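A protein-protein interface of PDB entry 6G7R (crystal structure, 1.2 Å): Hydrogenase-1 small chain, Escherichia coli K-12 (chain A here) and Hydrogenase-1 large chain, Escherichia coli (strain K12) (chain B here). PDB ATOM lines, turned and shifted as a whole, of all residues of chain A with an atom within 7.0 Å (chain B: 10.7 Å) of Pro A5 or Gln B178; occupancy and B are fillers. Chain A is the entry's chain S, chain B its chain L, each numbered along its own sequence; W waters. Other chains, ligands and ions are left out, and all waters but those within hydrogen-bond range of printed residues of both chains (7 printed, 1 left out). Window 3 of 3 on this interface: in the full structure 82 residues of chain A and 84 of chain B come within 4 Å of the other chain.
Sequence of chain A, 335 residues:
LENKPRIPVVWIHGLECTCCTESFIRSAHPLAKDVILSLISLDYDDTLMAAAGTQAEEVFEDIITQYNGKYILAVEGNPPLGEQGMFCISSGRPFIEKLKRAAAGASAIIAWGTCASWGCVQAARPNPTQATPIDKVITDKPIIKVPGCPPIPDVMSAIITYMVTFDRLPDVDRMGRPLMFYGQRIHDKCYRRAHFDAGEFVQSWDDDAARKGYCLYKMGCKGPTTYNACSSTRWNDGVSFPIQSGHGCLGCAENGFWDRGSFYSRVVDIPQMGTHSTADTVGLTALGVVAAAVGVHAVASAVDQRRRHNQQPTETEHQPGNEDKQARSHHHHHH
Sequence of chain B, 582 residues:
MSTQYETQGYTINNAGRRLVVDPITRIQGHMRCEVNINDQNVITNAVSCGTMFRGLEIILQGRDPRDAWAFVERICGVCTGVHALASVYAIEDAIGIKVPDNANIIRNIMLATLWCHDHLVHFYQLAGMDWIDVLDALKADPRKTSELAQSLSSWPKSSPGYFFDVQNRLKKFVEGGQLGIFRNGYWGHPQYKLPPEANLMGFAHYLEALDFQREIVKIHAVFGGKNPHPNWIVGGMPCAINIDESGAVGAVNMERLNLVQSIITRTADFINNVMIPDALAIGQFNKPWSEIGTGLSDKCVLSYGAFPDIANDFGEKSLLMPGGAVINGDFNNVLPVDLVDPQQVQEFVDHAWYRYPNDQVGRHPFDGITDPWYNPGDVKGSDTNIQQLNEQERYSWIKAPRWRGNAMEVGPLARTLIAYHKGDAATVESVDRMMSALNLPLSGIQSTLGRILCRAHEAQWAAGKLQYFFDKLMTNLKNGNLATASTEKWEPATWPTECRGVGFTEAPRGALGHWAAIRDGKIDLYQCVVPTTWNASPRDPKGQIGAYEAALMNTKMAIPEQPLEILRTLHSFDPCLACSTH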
ATOM      1  N   PRO A   5      11.624  -7.353 -21.347  1.00  0.00           N
ATOM      2  CA  PRO A   5      10.323  -7.666 -21.948  1.00  0.00           C
ATOM      3  C   PRO A   5      10.367  -7.620 -23.477  1.00  0.00           C
ATOM      4  O   PRO A   5      11.142  -6.873 -24.050  1.00  0.00           O
ATOM      5  CB  PRO A   5       9.351  -6.598 -21.420  1.00  0.00           C
ATOM      6  CG  PRO A   5      10.001  -6.112 -20.150  1.00  0.00           C
ATOM      7  CD  PRO A   5      11.494  -6.230 -20.401  1.00  0.00           C
ATOM      8  N   ARG A   6       9.556  -8.455 -24.099  1.00  0.00           N
ATOM      9  CA  ARG A   6       9.436  -8.513 -25.557  1.00  0.00           C
ATOM     10  C   ARG A   6       8.222  -7.694 -26.001  1.00  0.00           C
ATOM     11  O   ARG A   6       7.284  -7.534 -25.271  1.00  0.00           O
ATOM     12  CB  ARG A   6       9.370  -9.991 -25.949  1.00  0.00           C
ATOM     13  CG  ARG A   6      10.688 -10.741 -25.782  1.00  0.00           C
ATOM     14  CD  ARG A   6      10.539 -12.254 -25.810  1.00  0.00           C
ATOM     15  NE  ARG A   6      10.038 -12.838 -24.562  1.00  0.00           N
ATOM     16  CZ  ARG A   6       8.876 -13.466 -24.426  1.00  0.00           C
ATOM     17  NH1 ARG A   6       8.082 -13.614 -25.478  1.00  0.00           N
ATOM     18  NH2 ARG A   6       8.531 -13.945 -23.227  1.00  0.00           N
ATOM     19  N   ILE A   7       8.252  -7.222 -27.234  1.00  0.00           N
ATOM     20  CA  ILE A   7       7.196  -6.351 -27.737  1.00  0.00           C
ATOM     21  C   ILE A   7       5.905  -7.163 -27.906  1.00  0.00           C
ATOM     22  O   ILE A   7       5.916  -8.232 -28.545  1.00  0.00           O
ATOM     23  CB  ILE A   7       7.578  -5.685 -29.068  1.00  0.00           C
ATOM     24  CG1 ILE A   7       6.479  -4.726 -29.528  1.00  0.00           C
ATOM     25  CG2 ILE A   7       7.907  -6.704 -30.136  1.00  0.00           C
ATOM     26  CD1 ILE A   7       6.937  -3.651 -30.469  1.00  0.00           C
ATOM     27  N   PRO A   8       4.790  -6.669 -27.373  1.00  0.00           N
ATOM     28  CA  PRO A   8       3.545  -7.380 -27.526  1.00  0.00           C
ATOM     29  C   PRO A   8       3.014  -7.333 -28.965  1.00  0.00           C
ATOM     30  O   PRO A   8       2.991  -6.286 -29.591  1.00  0.00           O
ATOM     31  CB  PRO A   8       2.566  -6.696 -26.569  1.00  0.00           C
ATOM     32  CG  PRO A   8       3.264  -5.533 -25.987  1.00  0.00           C
ATOM     33  CD  PRO A   8       4.670  -5.515 -26.494  1.00  0.00           C
ATOM     34  N   ILE A  36       8.985 -16.398 -31.698  1.00  0.00           N
ATOM     35  CA  ILE A  36       7.945 -16.469 -30.645  1.00  0.00           C
ATOM     36  C   ILE A  36       8.629 -16.503 -29.268  1.00  0.00           C
ATOM     37  O   ILE A  36       8.129 -15.913 -28.304  1.00  0.00           O
ATOM     38  CB  ILE A  36       7.026 -17.701 -30.885  1.00  0.00           C
ATOM     39  CG1 ILE A  36       6.205 -17.447 -32.153  1.00  0.00           C
ATOM     40  CG2 ILE A  36       6.167 -18.042 -29.674  1.00  0.00           C
ATOM     41  CD1 ILE A  36       5.505 -18.667 -32.709  1.00  0.00           C
ATOM     42  N   LEU A  39      11.981 -13.046 -29.664  1.00  0.00           N
ATOM     43  CA  LEU A  39      12.020 -11.732 -30.313  1.00  0.00           C
ATOM     44  C   LEU A  39      10.766 -10.908 -30.028  1.00  0.00           C
ATOM     45  O   LEU A  39      10.902  -9.698 -29.897  1.00  0.00           O
ATOM     46  CB  LEU A  39      12.229 -11.881 -31.818  1.00  0.00           C
ATOM     47  CG  LEU A  39      13.526 -12.564 -32.229  1.00  0.00           C
ATOM     48  CD1 LEU A  39      13.662 -12.484 -33.739  1.00  0.00           C
ATOM     49  CD2 LEU A  39      14.736 -11.962 -31.524  1.00  0.00           C
ATOM     50  N   ILE A  40       9.597 -11.541 -29.980  1.00  0.00           N
ATOM     51  CA  ILE A  40       8.324 -10.839 -29.768  1.00  0.00           C
ATOM     52  C   ILE A  40       7.588 -11.576 -28.659  1.00  0.00           C
ATOM     53  O   ILE A  40       7.998 -12.649 -28.265  1.00  0.00           O
ATOM     54  CB  ILE A  40       7.442 -10.778 -31.044  1.00  0.00           C
ATOM     55  CG1 ILE A  40       6.955 -12.175 -31.492  1.00  0.00           C
ATOM     56  CG2 ILE A  40       8.170 -10.031 -32.152  1.00  0.00           C
ATOM     57  CD1 ILE A  40       5.966 -12.203 -32.632  1.00  0.00           C
ATOM     58  N   SER A  41       6.501 -10.976 -28.166  1.00  0.00           N
ATOM     59  CA  SER A  41       5.550 -11.699 -27.335  1.00  0.00           C
ATOM     60  C   SER A  41       4.261 -11.845 -28.140  1.00  0.00           C
ATOM     61  O   SER A  41       3.513 -10.885 -28.281  1.00  0.00           O
ATOM     62  CB  SER A  41       5.330 -11.017 -26.001  1.00  0.00           C
ATOM     63  OG  SER A  41       4.552 -11.819 -25.135  1.00  0.00           O
ATOM     64  N   LEU A  42       4.057 -13.036 -28.702  1.00  0.00           N
ATOM     65  CA  LEU A  42       2.874 -13.295 -29.509  1.00  0.00           C
ATOM     66  C   LEU A  42       1.754 -13.606 -28.528  1.00  0.00           C
ATOM     67  O   LEU A  42       1.614 -14.708 -28.044  1.00  0.00           O
ATOM     68  CB  LEU A  42       3.152 -14.426 -30.494  1.00  0.00           C
ATOM     69  CG  LEU A  42       2.001 -14.793 -31.420  1.00  0.00           C
ATOM     70  CD1 LEU A  42       1.549 -13.615 -32.272  1.00  0.00           C
ATOM     71  CD2 LEU A  42       2.374 -15.968 -32.315  1.00  0.00           C
ATOM     72  N   ASP A  43       0.976 -12.575 -28.238  1.00  0.00           N
ATOM     73  CA  ASP A  43       0.100 -12.589 -27.083  1.00  0.00           C
ATOM     74  C   ASP A  43      -1.320 -13.031 -27.436  1.00  0.00           C
ATOM     75  O   ASP A  43      -2.089 -13.332 -26.531  1.00  0.00           O
ATOM     76  CB  ASP A  43       0.073 -11.198 -26.452  1.00  0.00           C
ATOM     77  CG  ASP A  43       1.342 -10.861 -25.703  1.00  0.00           C
ATOM     78  OD1 ASP A  43       1.988 -11.811 -25.202  1.00  0.00           O
ATOM     79  OD2 ASP A  43       1.701  -9.659 -25.643  1.00  0.00           O
ATOM     80  N   TYR A  67      -1.710  -3.209 -22.708  1.00  0.00           N
ATOM     81  CA  TYR A  67      -0.703  -2.727 -23.626  1.00  0.00           C
ATOM     82  C   TYR A  67      -1.258  -1.710 -24.626  1.00  0.00           C
ATOM     83  O   TYR A  67      -0.642  -1.450 -25.659  1.00  0.00           O
ATOM     84  CB  TYR A  67      -0.032  -3.914 -24.312  1.00  0.00           C
ATOM     85  CG  TYR A  67       0.761  -4.770 -23.357  1.00  0.00           C
ATOM     86  CD1 TYR A  67       2.003  -4.344 -22.902  1.00  0.00           C
ATOM     87  CD2 TYR A  67       0.293  -5.991 -22.904  1.00  0.00           C
ATOM     88  CE1 TYR A  67       2.759  -5.112 -22.033  1.00  0.00           C
ATOM     89  CE2 TYR A  67       1.038  -6.774 -22.030  1.00  0.00           C
ATOM     90  CZ  TYR A  67       2.273  -6.330 -21.600  1.00  0.00           C
ATOM     91  OH  TYR A  67       2.996  -7.102 -20.739  1.00  0.00           O
ATOM     92  N   VAL B 134       1.698 -27.964 -20.614  1.00  0.00           N
ATOM     93  CA  VAL B 134       2.973 -27.309 -20.867  1.00  0.00           C
ATOM     94  C   VAL B 134       3.533 -26.736 -19.571  1.00  0.00           C
ATOM     95  O   VAL B 134       4.742 -26.854 -19.313  1.00  0.00           O
ATOM     96  CB  VAL B 134       2.816 -26.208 -21.927  1.00  0.00           C
ATOM     97  CG1 VAL B 134       4.063 -25.354 -22.061  1.00  0.00           C
ATOM     98  CG2 VAL B 134       2.453 -26.810 -23.273  1.00  0.00           C
ATOM     99  N   LEU B 135       2.704 -26.110 -18.754  1.00  0.00           N
ATOM    100  CA  LEU B 135       3.248 -25.470 -17.530  1.00  0.00           C
ATOM    101  C   LEU B 135       3.713 -26.534 -16.530  1.00  0.00           C
ATOM    102  O   LEU B 135       4.693 -26.317 -15.796  1.00  0.00           O
ATOM    103  CB  LEU B 135       2.211 -24.523 -16.925  1.00  0.00           C
ATOM    104  CG  LEU B 135       2.253 -23.092 -17.453  1.00  0.00           C
ATOM    105  CD1 LEU B 135       2.301 -23.047 -18.948  1.00  0.00           C
ATOM    106  CD2 LEU B 135       1.109 -22.262 -16.932  1.00  0.00           C
ATOM    107  N   ARG B 169      14.536 -22.884 -20.875  1.00  0.00           N
ATOM    108  CA  ARG B 169      14.042 -21.911 -21.862  1.00  0.00           C
ATOM    109  C   ARG B 169      12.569 -21.587 -21.558  1.00  0.00           C
ATOM    110  O   ARG B 169      12.152 -20.442 -21.610  1.00  0.00           O
ATOM    111  CB  ARG B 169      14.228 -22.469 -23.273  1.00  0.00           C
ATOM    112  CG  ARG B 169      13.760 -21.567 -24.405  1.00  0.00           C
ATOM    113  CD  ARG B 169      14.887 -21.103 -25.289  1.00  0.00           C
ATOM    114  NE  ARG B 169      14.421 -20.177 -26.313  1.00  0.00           N
ATOM    115  CZ  ARG B 169      14.604 -20.331 -27.618  1.00  0.00           C
ATOM    116  NH1 ARG B 169      14.976 -21.501 -28.119  1.00  0.00           N
ATOM    117  NH2 ARG B 169      14.455 -19.291 -28.410  1.00  0.00           N
ATOM    118  N   LEU B 170      11.787 -22.632 -21.245  1.00  0.00           N
ATOM    119  CA  LEU B 170      10.384 -22.405 -20.881  1.00  0.00           C
ATOM    120  C   LEU B 170      10.265 -21.589 -19.591  1.00  0.00           C
ATOM    121  O   LEU B 170       9.446 -20.663 -19.523  1.00  0.00           O
ATOM    122  CB  LEU B 170       9.661 -23.748 -20.772  1.00  0.00           C
ATOM    123  CG  LEU B 170       8.182 -23.677 -20.411  1.00  0.00           C
ATOM    124  CD1 LEU B 170       7.370 -22.920 -21.465  1.00  0.00           C
ATOM    125  CD2 LEU B 170       7.630 -25.085 -20.197  1.00  0.00           C
ATOM    126  N   LYS B 171      11.088 -21.922 -18.594  1.00  0.00           N
ATOM    127  CA  LYS B 171      11.028 -21.160 -17.343  1.00  0.00           C
ATOM    128  C   LYS B 171      11.292 -19.677 -17.602  1.00  0.00           C
ATOM    129  O   LYS B 171      10.580 -18.811 -17.077  1.00  0.00           O
ATOM    130  CB  LYS B 171      12.086 -21.730 -16.414  1.00  0.00           C
ATOM    131  CG  LYS B 171      12.252 -21.003 -15.102  1.00  0.00           C
ATOM    132  CD  LYS B 171      13.375 -21.617 -14.312  1.00  0.00           C
ATOM    133  CE  LYS B 171      13.755 -20.744 -13.165  1.00  0.00           C
ATOM    134  NZ  LYS B 171      14.849 -21.360 -12.404  1.00  0.00           N
ATOM    135  N   LYS B 172      12.325 -19.377 -18.369  1.00  0.00           N
ATOM    136  CA  LYS B 172      12.659 -17.965 -18.623  1.00  0.00           C
ATOM    137  C   LYS B 172      11.601 -17.272 -19.499  1.00  0.00           C
ATOM    138  O   LYS B 172      11.318 -16.085 -19.315  1.00  0.00           O
ATOM    139  CB  LYS B 172      14.062 -17.888 -19.222  1.00  0.00           C
ATOM    140  CG  LYS B 172      15.189 -18.171 -18.227  1.00  0.00           C
ATOM    141  CD  LYS B 172      15.147 -17.286 -16.973  1.00  0.00           C
ATOM    142  CE  LYS B 172      16.504 -16.868 -16.445  1.00  0.00           C
ATOM    143  NZ  LYS B 172      17.063 -17.878 -15.518  1.00  0.00           N
ATOM    144  N   PHE B 173      10.970 -18.014 -20.399  1.00  0.00           N
ATOM    145  CA  PHE B 173       9.861 -17.503 -21.209  1.00  0.00           C
ATOM    146  C   PHE B 173       8.683 -17.070 -20.329  1.00  0.00           C
ATOM    147  O   PHE B 173       8.117 -16.015 -20.579  1.00  0.00           O
ATOM    148  CB  PHE B 173       9.433 -18.573 -22.211  1.00  0.00           C
ATOM    149  CG  PHE B 173       8.282 -18.174 -23.101  1.00  0.00           C
ATOM    150  CD1 PHE B 173       8.514 -17.357 -24.196  1.00  0.00           C
ATOM    151  CD2 PHE B 173       6.999 -18.653 -22.891  1.00  0.00           C
ATOM    152  CE1 PHE B 173       7.484 -17.023 -25.050  1.00  0.00           C
ATOM    153  CE2 PHE B 173       5.961 -18.296 -23.737  1.00  0.00           C
ATOM    154  CZ  PHE B 173       6.212 -17.494 -24.824  1.00  0.00           C
ATOM    155  N   VAL B 174       8.344 -17.885 -19.332  1.00  0.00           N
ATOM    156  CA  VAL B 174       7.158 -17.709 -18.440  1.00  0.00           C
ATOM    157  C   VAL B 174       7.451 -16.649 -17.376  1.00  0.00           C
ATOM    158  O   VAL B 174       6.560 -15.959 -16.926  1.00  0.00           O
ATOM    159  CB  VAL B 174       6.744 -19.063 -17.797  1.00  0.00           C
ATOM    160  CG1 VAL B 174       5.748 -18.985 -16.642  1.00  0.00           C
ATOM    161  CG2 VAL B 174       6.232 -19.992 -18.894  1.00  0.00           C
ATOM    162  N   GLU B 175       8.689 -16.558 -16.937  1.00  0.00           N
ATOM    163  CA  GLU B 175       9.046 -15.876 -15.665  1.00  0.00           C
ATOM    164  C   GLU B 175       8.689 -14.391 -15.708  1.00  0.00           C
ATOM    165  O   GLU B 175       8.343 -13.832 -14.661  1.00  0.00           O
ATOM    166  CB  GLU B 175      10.543 -16.071 -15.430  1.00  0.00           C
ATOM    167  CG  GLU B 175      11.144 -15.268 -14.310  1.00  0.00           C
ATOM    168  CD  GLU B 175      12.614 -15.613 -14.164  1.00  0.00           C
ATOM    169  OE1 GLU B 175      12.918 -16.774 -13.755  1.00  0.00           O
ATOM    170  OE2 GLU B 175      13.446 -14.746 -14.519  1.00  0.00           O
ATOM    171  N   GLY B 176       8.866 -13.734 -16.854  1.00  0.00           N
ATOM    172  CA  GLY B 176       8.449 -12.311 -16.956  1.00  0.00           C
ATOM    173  C   GLY B 176       6.944 -12.072 -17.105  1.00  0.00           C
ATOM    174  O   GLY B 176       6.566 -10.906 -17.247  1.00  0.00           O
ATOM    175  N   GLY B 177       6.101 -13.118 -17.044  1.00  0.00           N
ATOM    176  CA  GLY B 177       4.647 -12.982 -17.176  1.00  0.00           C
ATOM    177  C   GLY B 177       4.154 -12.874 -18.604  1.00  0.00           C
ATOM    178  O   GLY B 177       2.932 -12.784 -18.819  1.00  0.00           O
ATOM    179  N   GLN B 178       5.047 -12.944 -19.593  1.00  0.00           N
ATOM    180  CA  GLN B 178       4.616 -12.848 -20.981  1.00  0.00           C
ATOM    181  C   GLN B 178       4.437 -14.271 -21.514  1.00  0.00           C
ATOM    182  O   GLN B 178       5.296 -14.797 -22.232  1.00  0.00           O
ATOM    183  CB  GLN B 178       5.626 -12.041 -21.794  1.00  0.00           C
ATOM    184  CG  GLN B 178       5.692 -10.565 -21.385  1.00  0.00           C
ATOM    185  CD  GLN B 178       6.556  -9.788 -22.353  1.00  0.00           C
ATOM    186  OE1 GLN B 178       7.766  -9.919 -22.371  1.00  0.00           O
ATOM    187  NE2 GLN B 178       5.932  -9.032 -23.239  1.00  0.00           N
ATOM    188  N   LEU B 179       3.314 -14.901 -21.177  1.00  0.00           N
ATOM    189  CA  LEU B 179       3.117 -16.324 -21.469  1.00  0.00           C
ATOM    190  C   LEU B 179       2.702 -16.580 -22.915  1.00  0.00           C
ATOM    191  O   LEU B 179       2.651 -17.748 -23.295  1.00  0.00           O
ATOM    192  CB  LEU B 179       2.087 -16.934 -20.518  1.00  0.00           C
ATOM    193  CG  LEU B 179       2.690 -17.581 -19.283  1.00  0.00           C
ATOM    194  CD1 LEU B 179       3.367 -16.526 -18.416  1.00  0.00           C
ATOM    195  CD2 LEU B 179       1.657 -18.353 -18.487  1.00  0.00           C
ATOM    196  N   GLY B 180       2.414 -15.542 -23.685  1.00  0.00           N
ATOM    197  CA  GLY B 180       2.133 -15.715 -25.093  1.00  0.00           C
ATOM    198  C   GLY B 180       0.990 -16.680 -25.359  1.00  0.00           C
ATOM    199  O   GLY B 180      -0.080 -16.597 -24.753  1.00  0.00           O
ATOM    200  N   ILE B 181       1.288 -17.675 -26.185  1.00  0.00           N
ATOM    201  CA  ILE B 181       0.283 -18.665 -26.565  1.00  0.00           C
ATOM    202  C   ILE B 181      -0.119 -19.561 -25.388  1.00  0.00           C
ATOM    203  O   ILE B 181      -1.104 -20.275 -25.524  1.00  0.00           O
ATOM    204  CB  ILE B 181       0.770 -19.517 -27.758  1.00  0.00           C
ATOM    205  CG1 ILE B 181       2.093 -20.226 -27.479  1.00  0.00           C
ATOM    206  CG2 ILE B 181       0.797 -18.691 -29.033  1.00  0.00           C
ATOM    207  CD1 ILE B 181       2.408 -21.332 -28.478  1.00  0.00           C
ATOM    208  N   PHE B 182       0.581 -19.511 -24.277  1.00  0.00           N
ATOM    209  CA  PHE B 182       0.175 -20.330 -23.117  1.00  0.00           C
ATOM    210  C   PHE B 182      -0.712 -19.560 -22.132  1.00  0.00           C
ATOM    211  O   PHE B 182      -1.179 -20.141 -21.150  1.00  0.00           O
ATOM    212  CB  PHE B 182       1.407 -20.844 -22.372  1.00  0.00           C
ATOM    213  CG  PHE B 182       2.408 -21.524 -23.255  1.00  0.00           C
ATOM    214  CD1 PHE B 182       2.007 -22.486 -24.162  1.00  0.00           C
ATOM    215  CD2 PHE B 182       3.738 -21.164 -23.207  1.00  0.00           C
ATOM    216  CE1 PHE B 182       2.929 -23.077 -25.018  1.00  0.00           C
ATOM    217  CE2 PHE B 182       4.664 -21.769 -24.037  1.00  0.00           C
ATOM    218  CZ  PHE B 182       4.254 -22.718 -24.948  1.00  0.00           C
ATOM    219  N   ARG B 183      -0.981 -18.280 -22.377  1.00  0.00           N
ATOM    220  CA  ARG B 183      -1.724 -17.506 -21.397  1.00  0.00           C
ATOM    221  C   ARG B 183      -3.173 -17.994 -21.268  1.00  0.00           C
ATOM    222  O   ARG B 183      -3.889 -18.244 -22.235  1.00  0.00           O
ATOM    223  CB  ARG B 183      -1.678 -16.027 -21.769  1.00  0.00           C
ATOM    224  CG  ARG B 183      -2.378 -15.125 -20.773  1.00  0.00           C
ATOM    225  CD  ARG B 183      -2.322 -13.678 -21.189  1.00  0.00           C
ATOM    226  NE  ARG B 183      -3.093 -12.869 -20.266  1.00  0.00           N
ATOM    227  CZ  ARG B 183      -2.634 -11.813 -19.600  1.00  0.00           C
ATOM    228  NH1 ARG B 183      -1.370 -11.442 -19.712  1.00  0.00           N
ATOM    229  NH2 ARG B 183      -3.448 -11.118 -18.818  1.00  0.00           N
ATOM    230  N   ASN B 184      -3.610 -18.068 -20.002  1.00  0.00           N
ATOM    231  CA  ASN B 184      -5.000 -18.373 -19.680  1.00  0.00           C
ATOM    232  C   ASN B 184      -5.447 -19.720 -20.266  1.00  0.00           C
ATOM    233  O   ASN B 184      -6.606 -19.923 -20.612  1.00  0.00           O
ATOM    234  CB  ASN B 184      -5.954 -17.257 -20.136  1.00  0.00           C
ATOM    235  CG  ASN B 184      -7.214 -17.198 -19.306  1.00  0.00           C
ATOM    236  OD1 ASN B 184      -7.252 -17.710 -18.186  1.00  0.00           O
ATOM    237  ND2 ASN B 184      -8.239 -16.575 -19.856  1.00  0.00           N
ATOM    238  N   TRP B 187      -4.281 -25.384 -18.051  1.00  0.00           N
ATOM    239  CA  TRP B 187      -3.248 -26.084 -17.296  1.00  0.00           C
ATOM    240  C   TRP B 187      -3.807 -26.424 -15.914  1.00  0.00           C
ATOM    241  O   TRP B 187      -4.405 -25.592 -15.250  1.00  0.00           O
ATOM    242  CB  TRP B 187      -2.014 -25.186 -17.203  1.00  0.00           C
ATOM    243  CG  TRP B 187      -1.685 -24.448 -18.464  1.00  0.00           C
ATOM    244  CD1 TRP B 187      -1.607 -23.097 -18.609  1.00  0.00           C
ATOM    245  CD2 TRP B 187      -1.457 -25.005 -19.766  1.00  0.00           C
ATOM    246  NE1 TRP B 187      -1.311 -22.771 -19.907  1.00  0.00           N
ATOM    247  CE2 TRP B 187      -1.233 -23.926 -20.644  1.00  0.00           C
ATOM    248  CE3 TRP B 187      -1.477 -26.288 -20.309  1.00  0.00           C
ATOM    249  CZ2 TRP B 187      -1.016 -24.095 -22.009  1.00  0.00           C
ATOM    250  CZ3 TRP B 187      -1.246 -26.460 -21.661  1.00  0.00           C
ATOM    251  CH2 TRP B 187      -0.994 -25.379 -22.498  1.00  0.00           C
HETATM  252  O   HOH W   1       3.392 -16.879 -27.905  1.00  0.00           O
HETATM  253  O   HOH W   2       2.331  -9.475 -19.759  1.00  0.00           O
HETATM  254  O   HOH W   3      -2.464 -16.374 -26.000  1.00  0.00           O
HETATM  255  O   HOH W   4      -1.028 -14.005 -24.193  1.00  0.00           O
HETATM  256  O   HOH W   5       3.001  -9.017 -23.525  1.00  0.00           O
HETATM  257  O   HOH W   6      11.055 -14.120 -21.434  1.00  0.00           O
HETATM  258  O   HOH W   7       5.396 -14.352 -25.008  1.00  0.00           O
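The backbone carbonyl oxygen (O) of Phe B173 sits at hydrogen-bond distance from the guanidinium group (NH2) of Arg A6, 3.4 Å away. The backbone carbonyl oxygen of Arg A6 sits at hydrogen-bond distance from the side-chain amide nitrogen of Gln B178 (2.9 Å).
O of Ile A40 lies within hydrogen-bond range of NH1 of Arg A6, 3.0 Å away. The backbone carbonyl oxygen (O) of Ile A7 is in hydrogen-bond range of the backbone NH (N) of Ser A41 (2.8 Å). The side-chain hydroxyl of Ser A41 sits at hydrogen-bond distance from the side-chain carboxylate of Asp A43 (2.6 Å).
Pro A5 touches Gln B178. Ile A36 touches Phe B173. Ser A41 touches Gln B178 (CB to NE2, 3.5 Å). O of Leu A42 touches CA of Gly B180 (3.2 Å). Ile B181 touches Leu A42. Asp A43 touches Gly B180 (OD1 to CA, 3.9 Å).
Of chain B, only Gln B178 (3.4 Å) comes within 4 Å of Pro A5. Of chain B, only Phe B173 (3.4 Å) and Gln B178 (2.9 Å) come within 4 Å of Arg A6. Printed residues of chain B within 4 Å of Leu A42: Gly B180 (3.2 Å) and Ile B181 (3.5 Å). Tyr A67 touches none of the printed residues of chain B. Gly B176 touches none of the printed residues of chain A. Gln B178 touches just these residues of chain A: Pro A5 (3.4 Å), Arg A6 (2.9 Å) and Ser A41 (3.5 Å). Of the printed residues of chain A, Gly B180 touches Leu A42 and Asp A43.
Printed residues of chain A that touch a printed residue of chain B: Pro A5, Arg A6, Ile A36, Ser A41, Leu A42 and Asp A43. Hydrophobic or aromatic side chains of chain A within 4 Å of the printed part of chain B: Pro A5. Along chain A the printed residues that touch a printed residue of chain B span positions 5 to 43. Among the printed residues, no Asp or Glu carboxylate lies within 4 Å of a Lys or Arg side-chain nitrogen of the other chain.
Water W5 lies within hydrogen-bond range of the side-chain carboxylate (OD2) of Asp A43 (2.6 Å), the side-chain amide nitrogen (NE2) of Gln B178 (2.9 Å) and the side-chain hydroxyl (OH) of Tyr A67 (3.4 Å). Water W2 lies within hydrogen-bond range of OH of Tyr A67 (2.7 Å) and O of Gly B177 (3.5 Å). Water W4 lies within hydrogen-bond range of the backbone carbonyl oxygen of Asp A43 (2.7 Å) and the backbone carbonyl oxygen of Gly B180 (2.8 Å). Water W7 lies within hydrogen-bond range of OG of Ser A41, O of Gln B178, NH1 of Arg A6 and N of Gly B180. Water W1 lies within hydrogen-bond range of the backbone carbonyl oxygen of Leu A42 and the backbone NH of Ile B181. Water W6 bridges O of Lys B172 (2.9 Å) and NH2 of Arg A6 (3.1 Å).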
